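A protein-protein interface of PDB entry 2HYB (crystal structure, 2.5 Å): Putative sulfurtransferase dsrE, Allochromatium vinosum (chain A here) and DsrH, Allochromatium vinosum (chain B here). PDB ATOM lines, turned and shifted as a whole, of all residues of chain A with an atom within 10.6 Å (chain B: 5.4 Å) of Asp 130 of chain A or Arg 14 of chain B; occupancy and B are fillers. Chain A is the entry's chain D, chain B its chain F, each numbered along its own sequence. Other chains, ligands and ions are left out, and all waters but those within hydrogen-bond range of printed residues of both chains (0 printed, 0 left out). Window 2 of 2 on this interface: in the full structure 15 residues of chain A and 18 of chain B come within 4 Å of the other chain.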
ATOM      1  N   GLN A   6      15.861 -21.928 -10.895  1.00  0.00           N
ATOM      2  CA  GLN A   6      15.889 -20.470 -10.919  1.00  0.00           C
ATOM      3  C   GLN A   6      14.872 -19.996 -11.955  1.00  0.00           C
ATOM      4  O   GLN A   6      14.850 -20.499 -13.071  1.00  0.00           O
ATOM      5  CB  GLN A   6      17.286 -19.975 -11.300  1.00  0.00           C
ATOM      6  CG  GLN A   6      17.518 -18.488 -11.084  1.00  0.00           C
ATOM      7  CD  GLN A   6      18.930 -18.078 -11.462  1.00  0.00           C
ATOM      8  OE1 GLN A   6      19.906 -18.726 -11.070  1.00  0.00           O
ATOM      9  NE2 GLN A   6      19.047 -17.005 -12.228  1.00  0.00           N
ATOM     10  N   ILE A   7      14.025 -19.044 -11.587  1.00  0.00           N
ATOM     11  CA  ILE A   7      13.016 -18.528 -12.513  1.00  0.00           C
ATOM     12  C   ILE A   7      13.200 -17.026 -12.698  1.00  0.00           C
ATOM     13  O   ILE A   7      13.079 -16.253 -11.740  1.00  0.00           O
ATOM     14  CB  ILE A   7      11.593 -18.821 -12.001  1.00  0.00           C
ATOM     15  CG1 ILE A   7      11.401 -20.333 -11.908  1.00  0.00           C
ATOM     16  CG2 ILE A   7      10.563 -18.203 -12.922  1.00  0.00           C
ATOM     17  CD1 ILE A   7      10.216 -20.746 -11.080  1.00  0.00           C
ATOM     18  N   ASN A   8      13.462 -16.610 -13.932  1.00  0.00           N
ATOM     19  CA  ASN A   8      13.730 -15.203 -14.195  1.00  0.00           C
ATOM     20  C   ASN A   8      12.625 -14.359 -14.769  1.00  0.00           C
ATOM     21  O   ASN A   8      12.800 -13.148 -14.932  1.00  0.00           O
ATOM     22  CB  ASN A   8      14.949 -15.061 -15.111  1.00  0.00           C
ATOM     23  CG  ASN A   8      16.142 -15.865 -14.630  1.00  0.00           C
ATOM     24  OD1 ASN A   8      16.324 -16.066 -13.425  1.00  0.00           O
ATOM     25  ND2 ASN A   8      16.965 -16.327 -15.569  1.00  0.00           N
ATOM     26  N   GLU A   9      11.483 -14.950 -15.080  1.00  0.00           N
ATOM     27  CA  GLU A   9      10.432 -14.134 -15.664  1.00  0.00           C
ATOM     28  C   GLU A   9       9.124 -14.158 -14.890  1.00  0.00           C
ATOM     29  O   GLU A   9       8.866 -15.053 -14.088  1.00  0.00           O
ATOM     30  CB  GLU A   9      10.219 -14.563 -17.111  1.00  0.00           C
ATOM     31  CG  GLU A   9      11.499 -14.549 -17.945  1.00  0.00           C
ATOM     32  CD  GLU A   9      12.161 -13.171 -18.030  1.00  0.00           C
ATOM     33  OE1 GLU A   9      11.446 -12.140 -18.110  1.00  0.00           O
ATOM     34  OE2 GLU A   9      13.410 -13.123 -18.044  1.00  0.00           O
ATOM     35  N   GLY A  10       8.310 -13.139 -15.117  1.00  0.00           N
ATOM     36  CA  GLY A  10       7.037 -13.051 -14.441  1.00  0.00           C
ATOM     37  C   GLY A  10       6.048 -14.018 -15.053  1.00  0.00           C
ATOM     38  O   GLY A  10       6.321 -14.603 -16.106  1.00  0.00           O
ATOM     39  N   TYR A  12       2.767 -15.574 -17.038  1.00  0.00           N
ATOM     40  CA  TYR A  12       2.008 -15.340 -18.282  1.00  0.00           C
ATOM     41  C   TYR A  12       2.710 -14.620 -19.431  1.00  0.00           C
ATOM     42  O   TYR A  12       2.496 -14.946 -20.597  1.00  0.00           O
ATOM     43  CB  TYR A  12       0.688 -14.605 -17.985  1.00  0.00           C
ATOM     44  CG  TYR A  12      -0.212 -15.308 -16.993  1.00  0.00           C
ATOM     45  CD1 TYR A  12      -0.226 -14.928 -15.648  1.00  0.00           C
ATOM     46  CD2 TYR A  12      -1.012 -16.389 -17.387  1.00  0.00           C
ATOM     47  CE1 TYR A  12      -1.010 -15.605 -14.713  1.00  0.00           C
ATOM     48  CE2 TYR A  12      -1.798 -17.084 -16.458  1.00  0.00           C
ATOM     49  CZ  TYR A  12      -1.786 -16.683 -15.122  1.00  0.00           C
ATOM     50  OH  TYR A  12      -2.513 -17.376 -14.190  1.00  0.00           O
ATOM     51  N   GLN A  13       3.534 -13.640 -19.103  1.00  0.00           N
ATOM     52  CA  GLN A  13       4.254 -12.863 -20.106  1.00  0.00           C
ATOM     53  C   GLN A  13       5.245 -13.758 -20.855  1.00  0.00           C
ATOM     54  O   GLN A  13       5.400 -13.648 -22.077  1.00  0.00           O
ATOM     55  CB  GLN A  13       4.991 -11.702 -19.417  1.00  0.00           C
ATOM     56  CG  GLN A  13       5.633 -10.701 -20.346  1.00  0.00           C
ATOM     57  CD  GLN A  13       4.684  -9.604 -20.785  1.00  0.00           C
ATOM     58  OE1 GLN A  13       3.482  -9.688 -20.564  1.00  0.00           O
ATOM     59  NE2 GLN A  13       5.225  -8.566 -21.410  1.00  0.00           N
ATOM     60  N   HIS A  14       5.909 -14.644 -20.114  1.00  0.00           N
ATOM     61  CA  HIS A  14       6.887 -15.569 -20.683  1.00  0.00           C
ATOM     62  C   HIS A  14       6.569 -16.954 -20.136  1.00  0.00           C
ATOM     63  O   HIS A  14       6.122 -17.080 -19.002  1.00  0.00           O
ATOM     64  CB  HIS A  14       8.327 -15.181 -20.296  1.00  0.00           C
ATOM     65  CG  HIS A  14       8.784 -13.860 -20.845  1.00  0.00           C
ATOM     66  ND1 HIS A  14       8.625 -12.671 -20.161  1.00  0.00           N
ATOM     67  CD2 HIS A  14       9.404 -13.539 -22.007  1.00  0.00           C
ATOM     68  CE1 HIS A  14       9.130 -11.677 -20.874  1.00  0.00           C
ATOM     69  NE2 HIS A  14       9.610 -12.176 -21.999  1.00  0.00           N
ATOM     70  N   GLN A  15       6.817 -17.986 -20.936  1.00  0.00           N
ATOM     71  CA  GLN A  15       6.522 -19.360 -20.543  1.00  0.00           C
ATOM     72  C   GLN A  15       7.384 -19.903 -19.400  1.00  0.00           C
ATOM     73  O   GLN A  15       6.978 -20.849 -18.714  1.00  0.00           O
ATOM     74  CB  GLN A  15       6.648 -20.302 -21.759  1.00  0.00           C
ATOM     75  CG  GLN A  15       5.854 -21.613 -21.608  1.00  0.00           C
ATOM     76  CD  GLN A  15       6.120 -22.646 -22.710  1.00  0.00           C
ATOM     77  OE1 GLN A  15       6.392 -22.293 -23.867  1.00  0.00           O
ATOM     78  NE2 GLN A  15       6.012 -23.931 -22.355  1.00  0.00           N
ATOM     79  N   ALA A  16       8.559 -19.309 -19.192  1.00  0.00           N
ATOM     80  CA  ALA A  16       9.492 -19.745 -18.149  1.00  0.00           C
ATOM     81  C   ALA A  16       8.880 -20.369 -16.884  1.00  0.00           C
ATOM     82  O   ALA A  16       9.210 -21.501 -16.527  1.00  0.00           O
ATOM     83  CB  ALA A  16      10.425 -18.574 -17.757  1.00  0.00           C
ATOM     84  N   SER A  17       7.996 -19.644 -16.200  1.00  0.00           N
ATOM     85  CA  SER A  17       7.400 -20.171 -14.968  1.00  0.00           C
ATOM     86  C   SER A  17       6.601 -21.447 -15.222  1.00  0.00           C
ATOM     87  O   SER A  17       6.724 -22.420 -14.471  1.00  0.00           O
ATOM     88  CB  SER A  17       6.520 -19.106 -14.295  1.00  0.00           C
ATOM     89  OG  SER A  17       6.120 -19.496 -12.995  1.00  0.00           O
ATOM     90  N   SER A  19       7.017 -23.589 -17.606  1.00  0.00           N
ATOM     91  CA  SER A  19       7.978 -24.659 -17.898  1.00  0.00           C
ATOM     92  C   SER A  19       8.655 -25.153 -16.622  1.00  0.00           C
ATOM     93  O   SER A  19       8.812 -26.358 -16.419  1.00  0.00           O
ATOM     94  CB  SER A  19       9.055 -24.177 -18.873  1.00  0.00           C
ATOM     95  OG  SER A  19       8.487 -23.779 -20.095  1.00  0.00           O
ATOM     96  N   ALA A  20       9.057 -24.214 -15.770  1.00  0.00           N
ATOM     97  CA  ALA A  20       9.714 -24.556 -14.513  1.00  0.00           C
ATOM     98  C   ALA A  20       8.772 -25.401 -13.654  1.00  0.00           C
ATOM     99  O   ALA A  20       9.180 -26.395 -13.045  1.00  0.00           O
ATOM    100  CB  ALA A  20      10.116 -23.283 -13.767  1.00  0.00           C
ATOM    101  N   TYR A  40      13.987 -14.704  -9.437  1.00  0.00           N
ATOM    102  CA  TYR A  40      14.821 -13.517  -9.615  1.00  0.00           C
ATOM    103  C   TYR A  40      14.288 -12.706 -10.788  1.00  0.00           C
ATOM    104  O   TYR A  40      13.531 -13.224 -11.615  1.00  0.00           O
ATOM    105  CB  TYR A  40      16.268 -13.941  -9.877  1.00  0.00           C
ATOM    106  CG  TYR A  40      17.310 -12.854  -9.747  1.00  0.00           C
ATOM    107  CD1 TYR A  40      17.352 -12.033  -8.624  1.00  0.00           C
ATOM    108  CD2 TYR A  40      18.310 -12.697 -10.714  1.00  0.00           C
ATOM    109  CE1 TYR A  40      18.361 -11.094  -8.457  1.00  0.00           C
ATOM    110  CE2 TYR A  40      19.324 -11.755 -10.555  1.00  0.00           C
ATOM    111  CZ  TYR A  40      19.344 -10.960  -9.420  1.00  0.00           C
ATOM    112  OH  TYR A  40      20.359 -10.055  -9.226  1.00  0.00           O
ATOM    113  N   HIS A  41      14.692 -11.441 -10.863  1.00  0.00           N
ATOM    114  CA  HIS A  41      14.240 -10.537 -11.916  1.00  0.00           C
ATOM    115  C   HIS A  41      12.727 -10.415 -11.785  1.00  0.00           C
ATOM    116  O   HIS A  41      12.212 -10.337 -10.678  1.00  0.00           O
ATOM    117  CB  HIS A  41      14.592 -11.077 -13.309  1.00  0.00           C
ATOM    118  CG  HIS A  41      16.054 -11.312 -13.518  1.00  0.00           C
ATOM    119  ND1 HIS A  41      16.997 -10.312 -13.394  1.00  0.00           N
ATOM    120  CD2 HIS A  41      16.740 -12.432 -13.853  1.00  0.00           C
ATOM    121  CE1 HIS A  41      18.194 -10.804 -13.646  1.00  0.00           C
ATOM    122  NE2 HIS A  41      18.067 -12.090 -13.927  1.00  0.00           N
ATOM    123  N   ASP A  42      12.025 -10.395 -12.913  1.00  0.00           N
ATOM    124  CA  ASP A  42      10.569 -10.318 -12.931  1.00  0.00           C
ATOM    125  C   ASP A  42      10.011 -11.605 -12.364  1.00  0.00           C
ATOM    126  O   ASP A  42       8.822 -11.706 -12.110  1.00  0.00           O
ATOM    127  CB  ASP A  42      10.048 -10.163 -14.357  1.00  0.00           C
ATOM    128  CG  ASP A  42       9.938  -8.721 -14.780  1.00  0.00           C
ATOM    129  OD1 ASP A  42      10.311  -7.831 -13.984  1.00  0.00           O
ATOM    130  OD2 ASP A  42       9.469  -8.476 -15.910  1.00  0.00           O
ATOM    131  N   GLY A  43      10.870 -12.599 -12.191  1.00  0.00           N
ATOM    132  CA  GLY A  43      10.424 -13.853 -11.632  1.00  0.00           C
ATOM    133  C   GLY A  43       9.697 -13.616 -10.320  1.00  0.00           C
ATOM    134  O   GLY A  43       8.678 -14.251 -10.065  1.00  0.00           O
ATOM    135  N   VAL A 127      17.886 -23.402 -14.927  1.00  0.00           N
ATOM    136  CA  VAL A 127      17.378 -22.044 -15.058  1.00  0.00           C
ATOM    137  C   VAL A 127      16.400 -21.898 -16.222  1.00  0.00           C
ATOM    138  O   VAL A 127      16.664 -22.343 -17.351  1.00  0.00           O
ATOM    139  CB  VAL A 127      18.527 -21.034 -15.238  1.00  0.00           C
ATOM    140  CG1 VAL A 127      17.978 -19.620 -15.252  1.00  0.00           C
ATOM    141  CG2 VAL A 127      19.539 -21.200 -14.109  1.00  0.00           C
ATOM    142  N   PHE A 128      15.265 -21.272 -15.912  1.00  0.00           N
ATOM    143  CA  PHE A 128      14.185 -21.022 -16.849  1.00  0.00           C
ATOM    144  C   PHE A 128      13.969 -19.522 -17.029  1.00  0.00           C
ATOM    145  O   PHE A 128      13.499 -18.842 -16.109  1.00  0.00           O
ATOM    146  CB  PHE A 128      12.886 -21.616 -16.322  1.00  0.00           C
ATOM    147  CG  PHE A 128      12.910 -23.102 -16.153  1.00  0.00           C
ATOM    148  CD1 PHE A 128      13.344 -23.672 -14.961  1.00  0.00           C
ATOM    149  CD2 PHE A 128      12.490 -23.933 -17.198  1.00  0.00           C
ATOM    150  CE1 PHE A 128      13.353 -25.056 -14.811  1.00  0.00           C
ATOM    151  CE2 PHE A 128      12.497 -25.301 -17.063  1.00  0.00           C
ATOM    152  CZ  PHE A 128      12.929 -25.875 -15.866  1.00  0.00           C
ATOM    153  N   GLY A 129      14.280 -19.001 -18.212  1.00  0.00           N
ATOM    154  CA  GLY A 129      14.088 -17.582 -18.439  1.00  0.00           C
ATOM    155  C   GLY A 129      13.650 -17.246 -19.849  1.00  0.00           C
ATOM    156  O   GLY A 129      12.997 -18.044 -20.533  1.00  0.00           O
ATOM    157  N   ASP A 130      14.024 -16.048 -20.283  1.00  0.00           N
ATOM    158  CA  ASP A 130      13.695 -15.543 -21.611  1.00  0.00           C
ATOM    159  C   ASP A 130      14.731 -16.042 -22.618  1.00  0.00           C
ATOM    160  O   ASP A 130      15.810 -15.472 -22.743  1.00  0.00           O
ATOM    161  CB  ASP A 130      13.682 -14.008 -21.574  1.00  0.00           C
ATOM    162  CG  ASP A 130      12.896 -13.396 -22.713  1.00  0.00           C
ATOM    163  OD1 ASP A 130      12.706 -12.160 -22.710  1.00  0.00           O
ATOM    164  OD2 ASP A 130      12.470 -14.141 -23.615  1.00  0.00           O
ATOM    165  N   ASN B   8      15.605 -22.316 -25.553  1.00  0.00           N
ATOM    166  CA  ASN B   8      14.169 -22.062 -25.485  1.00  0.00           C
ATOM    167  C   ASN B   8      13.658 -21.013 -26.463  1.00  0.00           C
ATOM    168  O   ASN B   8      12.491 -20.616 -26.390  1.00  0.00           O
ATOM    169  CB  ASN B   8      13.774 -21.631 -24.070  1.00  0.00           C
ATOM    170  CG  ASN B   8      14.296 -20.244 -23.714  1.00  0.00           C
ATOM    171  OD1 ASN B   8      13.756 -19.573 -22.837  1.00  0.00           O
ATOM    172  ND2 ASN B   8      15.354 -19.812 -24.393  1.00  0.00           N
ATOM    173  N   LYS B   9      14.509 -20.568 -27.380  1.00  0.00           N
ATOM    174  CA  LYS B   9      14.090 -19.547 -28.331  1.00  0.00           C
ATOM    175  C   LYS B   9      14.154 -19.971 -29.795  1.00  0.00           C
ATOM    176  O   LYS B   9      14.973 -20.802 -30.187  1.00  0.00           O
ATOM    177  CB  LYS B   9      14.912 -18.266 -28.120  1.00  0.00           C
ATOM    178  CG  LYS B   9      14.122 -17.111 -27.515  1.00  0.00           C
ATOM    179  CD  LYS B   9      13.415 -17.526 -26.239  1.00  0.00           C
ATOM    180  CE  LYS B   9      12.501 -16.417 -25.725  1.00  0.00           C
ATOM    181  NZ  LYS B   9      11.361 -16.106 -26.643  1.00  0.00           N
ATOM    182  N   SER B  10      13.264 -19.374 -30.582  1.00  0.00           N
ATOM    183  CA  SER B  10      13.125 -19.609 -32.017  1.00  0.00           C
ATOM    184  C   SER B  10      14.442 -19.272 -32.728  1.00  0.00           C
ATOM    185  O   SER B  10      15.056 -18.244 -32.438  1.00  0.00           O
ATOM    186  CB  SER B  10      11.980 -18.714 -32.532  1.00  0.00           C
ATOM    187  OG  SER B  10      11.667 -18.917 -33.896  1.00  0.00           O
ATOM    188  N   PRO B  11      14.895 -20.132 -33.664  1.00  0.00           N
ATOM    189  CA  PRO B  11      16.140 -19.899 -34.399  1.00  0.00           C
ATOM    190  C   PRO B  11      15.947 -18.857 -35.478  1.00  0.00           C
ATOM    191  O   PRO B  11      16.891 -18.484 -36.162  1.00  0.00           O
ATOM    192  CB  PRO B  11      16.439 -21.262 -34.993  1.00  0.00           C
ATOM    193  CG  PRO B  11      15.079 -21.760 -35.316  1.00  0.00           C
ATOM    194  CD  PRO B  11      14.326 -21.437 -34.047  1.00  0.00           C
ATOM    195  N   PHE B  12      14.715 -18.395 -35.641  1.00  0.00           N
ATOM    196  CA  PHE B  12      14.439 -17.396 -36.656  1.00  0.00           C
ATOM    197  C   PHE B  12      14.289 -16.039 -35.993  1.00  0.00           C
ATOM    198  O   PHE B  12      14.165 -15.014 -36.673  1.00  0.00           O
ATOM    199  CB  PHE B  12      13.166 -17.749 -37.433  1.00  0.00           C
ATOM    200  CG  PHE B  12      13.098 -19.185 -37.853  1.00  0.00           C
ATOM    201  CD1 PHE B  12      12.315 -20.091 -37.145  1.00  0.00           C
ATOM    202  CD2 PHE B  12      13.852 -19.649 -38.916  1.00  0.00           C
ATOM    203  CE1 PHE B  12      12.287 -21.444 -37.483  1.00  0.00           C
ATOM    204  CE2 PHE B  12      13.833 -21.005 -39.261  1.00  0.00           C
ATOM    205  CZ  PHE B  12      13.048 -21.901 -38.542  1.00  0.00           C
ATOM    206  N   GLU B  13      14.298 -16.031 -34.661  1.00  0.00           N
ATOM    207  CA  GLU B  13      14.176 -14.788 -33.895  1.00  0.00           C
ATOM    208  C   GLU B  13      15.428 -14.471 -33.057  1.00  0.00           C
ATOM    209  O   GLU B  13      15.800 -13.309 -32.913  1.00  0.00           O
ATOM    210  CB  GLU B  13      12.947 -14.848 -32.974  1.00  0.00           C
ATOM    211  CG  GLU B  13      12.928 -13.765 -31.889  1.00  0.00           C
ATOM    212  CD  GLU B  13      11.637 -13.722 -31.077  1.00  0.00           C
ATOM    213  OE1 GLU B  13      11.658 -13.157 -29.963  1.00  0.00           O
ATOM    214  OE2 GLU B  13      10.601 -14.236 -31.556  1.00  0.00           O
ATOM    215  N   ARG B  14      16.070 -15.507 -32.519  1.00  0.00           N
ATOM    216  CA  ARG B  14      17.257 -15.351 -31.681  1.00  0.00           C
ATOM    217  C   ARG B  14      18.463 -16.126 -32.212  1.00  0.00           C
ATOM    218  O   ARG B  14      18.328 -17.092 -32.967  1.00  0.00           O
ATOM    219  CB  ARG B  14      16.967 -15.841 -30.262  1.00  0.00           C
ATOM    220  CG  ARG B  14      16.951 -14.772 -29.193  1.00  0.00           C
ATOM    221  CD  ARG B  14      15.570 -14.198 -29.010  1.00  0.00           C
ATOM    222  NE  ARG B  14      15.420 -13.582 -27.695  1.00  0.00           N
ATOM    223  CZ  ARG B  14      14.257 -13.202 -27.177  1.00  0.00           C
ATOM    224  NH1 ARG B  14      13.137 -13.375 -27.862  1.00  0.00           N
ATOM    225  NH2 ARG B  14      14.215 -12.659 -25.967  1.00  0.00           N
ATOM    226  N   ASN B  15      19.640 -15.704 -31.763  1.00  0.00           N
ATOM    227  CA  ASN B  15      20.908 -16.302 -32.155  1.00  0.00           C
ATOM    228  C   ASN B  15      21.323 -17.397 -31.164  1.00  0.00           C
ATOM    229  O   ASN B  15      22.388 -18.009 -31.303  1.00  0.00           O
ATOM    230  CB  ASN B  15      21.987 -15.218 -32.195  1.00  0.00           C
ATOM    231  CG  ASN B  15      22.305 -14.659 -30.809  1.00  0.00           C
ATOM    232  OD1 ASN B  15      21.433 -14.115 -30.123  1.00  0.00           O
ATOM    233  ND2 ASN B  15      23.558 -14.800 -30.388  1.00  0.00           N
ATOM    234  N   SER B  16      20.472 -17.650 -30.173  1.00  0.00           N
ATOM    235  CA  SER B  16      20.774 -18.644 -29.142  1.00  0.00           C
ATOM    236  C   SER B  16      21.038 -20.059 -29.652  1.00  0.00           C
ATOM    237  O   SER B  16      21.911 -20.752 -29.135  1.00  0.00           O
ATOM    238  CB  SER B  16      19.652 -18.677 -28.094  1.00  0.00           C
ATOM    239  OG  SER B  16      19.476 -17.404 -27.491  1.00  0.00           O
ATOM    240  N   LEU B  17      20.284 -20.491 -30.656  1.00  0.00           N
ATOM    241  CA  LEU B  17      20.473 -21.832 -31.187  1.00  0.00           C
ATOM    242  C   LEU B  17      21.854 -21.919 -31.821  1.00  0.00           C
ATOM    243  O   LEU B  17      22.582 -22.881 -31.583  1.00  0.00           O
ATOM    244  CB  LEU B  17      19.387 -22.172 -32.219  1.00  0.00           C
ATOM    245  CG  LEU B  17      19.199 -23.645 -32.639  1.00  0.00           C
ATOM    246  CD1 LEU B  17      19.577 -23.818 -34.087  1.00  0.00           C
ATOM    247  CD2 LEU B  17      20.005 -24.581 -31.729  1.00  0.00           C
ATOM    248  N   LEU B 102      19.557 -18.595 -23.119  1.00  0.00           N
ATOM    249  CA  LEU B 102      18.394 -17.717 -23.149  1.00  0.00           C
ATOM    250  C   LEU B 102      18.365 -16.727 -24.311  1.00  0.00           C
ATOM    251  O   LEU B 102      17.259 -16.412 -24.813  1.00  0.00           O
ATOM    252  CB  LEU B 102      18.315 -16.957 -21.821  1.00  0.00           C
ATOM    253  CG  LEU B 102      17.752 -17.635 -20.569  1.00  0.00           C
ATOM    254  CD1 LEU B 102      18.035 -19.116 -20.594  1.00  0.00           C
ATOM    255  CD2 LEU B 102      18.344 -16.974 -19.328  1.00  0.00           C
ATOM    256  OXT LEU B 102      19.451 -16.238 -24.682  1.00  0.00           O
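Of chain B, only Asn 8 (3.7 Å), Lys 9 (3.1 Å), Arg 14 (3.3 Å) and Leu 102 (2.7 Å) come within 4 Å of Asp 130 of chain A.
Arg 14 of chain B touches one residue of chain A.
Pro 11 of chain B touches none of the printed residues of chain A.
No residue of chain A comes within 4 Å of Glu 13 of chain B.
No residue of chain A comes within 4 Å of Asn 15 of chain B.
No residue of chain A comes within 4 Å of Ser 16 of chain B.
Of chain A, only Asp 130 (2.7 Å) comes within 4 Å of Leu 102 of chain B.
Printed residues of chain B within 4 Å of Gly 129 of chain A: Asn 8.
Of the printed residues of chain A, Asn 8 of chain B touches Gly 129 and Asp 130.
Gln 13 of chain A touches none of the printed residues of chain B.
The nearest residue of chain A that does not touch Arg 14 of chain B is His 14 of chain A (6.1 Å).
The side-chain carboxylate of Asp 130 of chain A sits at hydrogen-bond distance from a ring nitrogen (NE2) of His 14 of chain A (3.2 Å).
OE1 of Glu 13 of chain B lies within salt-bridge range of NH1 of Arg 14 of chain B (2.6 Å).
OG of Ser 16 of chain B sits at hydrogen-bond distance from OXT of Leu 102 of chain B (3.0 Å).
The backbone carbonyl oxygen of Gly 129 of chain A lies close to the side-chain amide oxygen of Asn 8 of chain B (2.9 Å).
The side-chain carboxylate of Asp 130 of chain A is in salt-bridge range of the side-chain amino group of Lys 9 of chain B.
The side-chain carboxylate of Asp 130 of chain A lies within salt-bridge range of the guanidinium group of Arg 14 of chain B, 3.3 Å away.
The backbone carbonyl oxygen (O) of Asp 130 of chain A lies close to the chain-end carboxylate (O) of Leu 102 of chain B.
Asn 8 of chain B touches Asp 130 of chain A.
Along chain B the printed residues that touch a printed residue of chain A span positions 8 to 102.
Along chain A the printed residues that touch a printed residue of chain B span positions 129 to 130.
Among the printed residues, 5 pairs touch across the chains.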
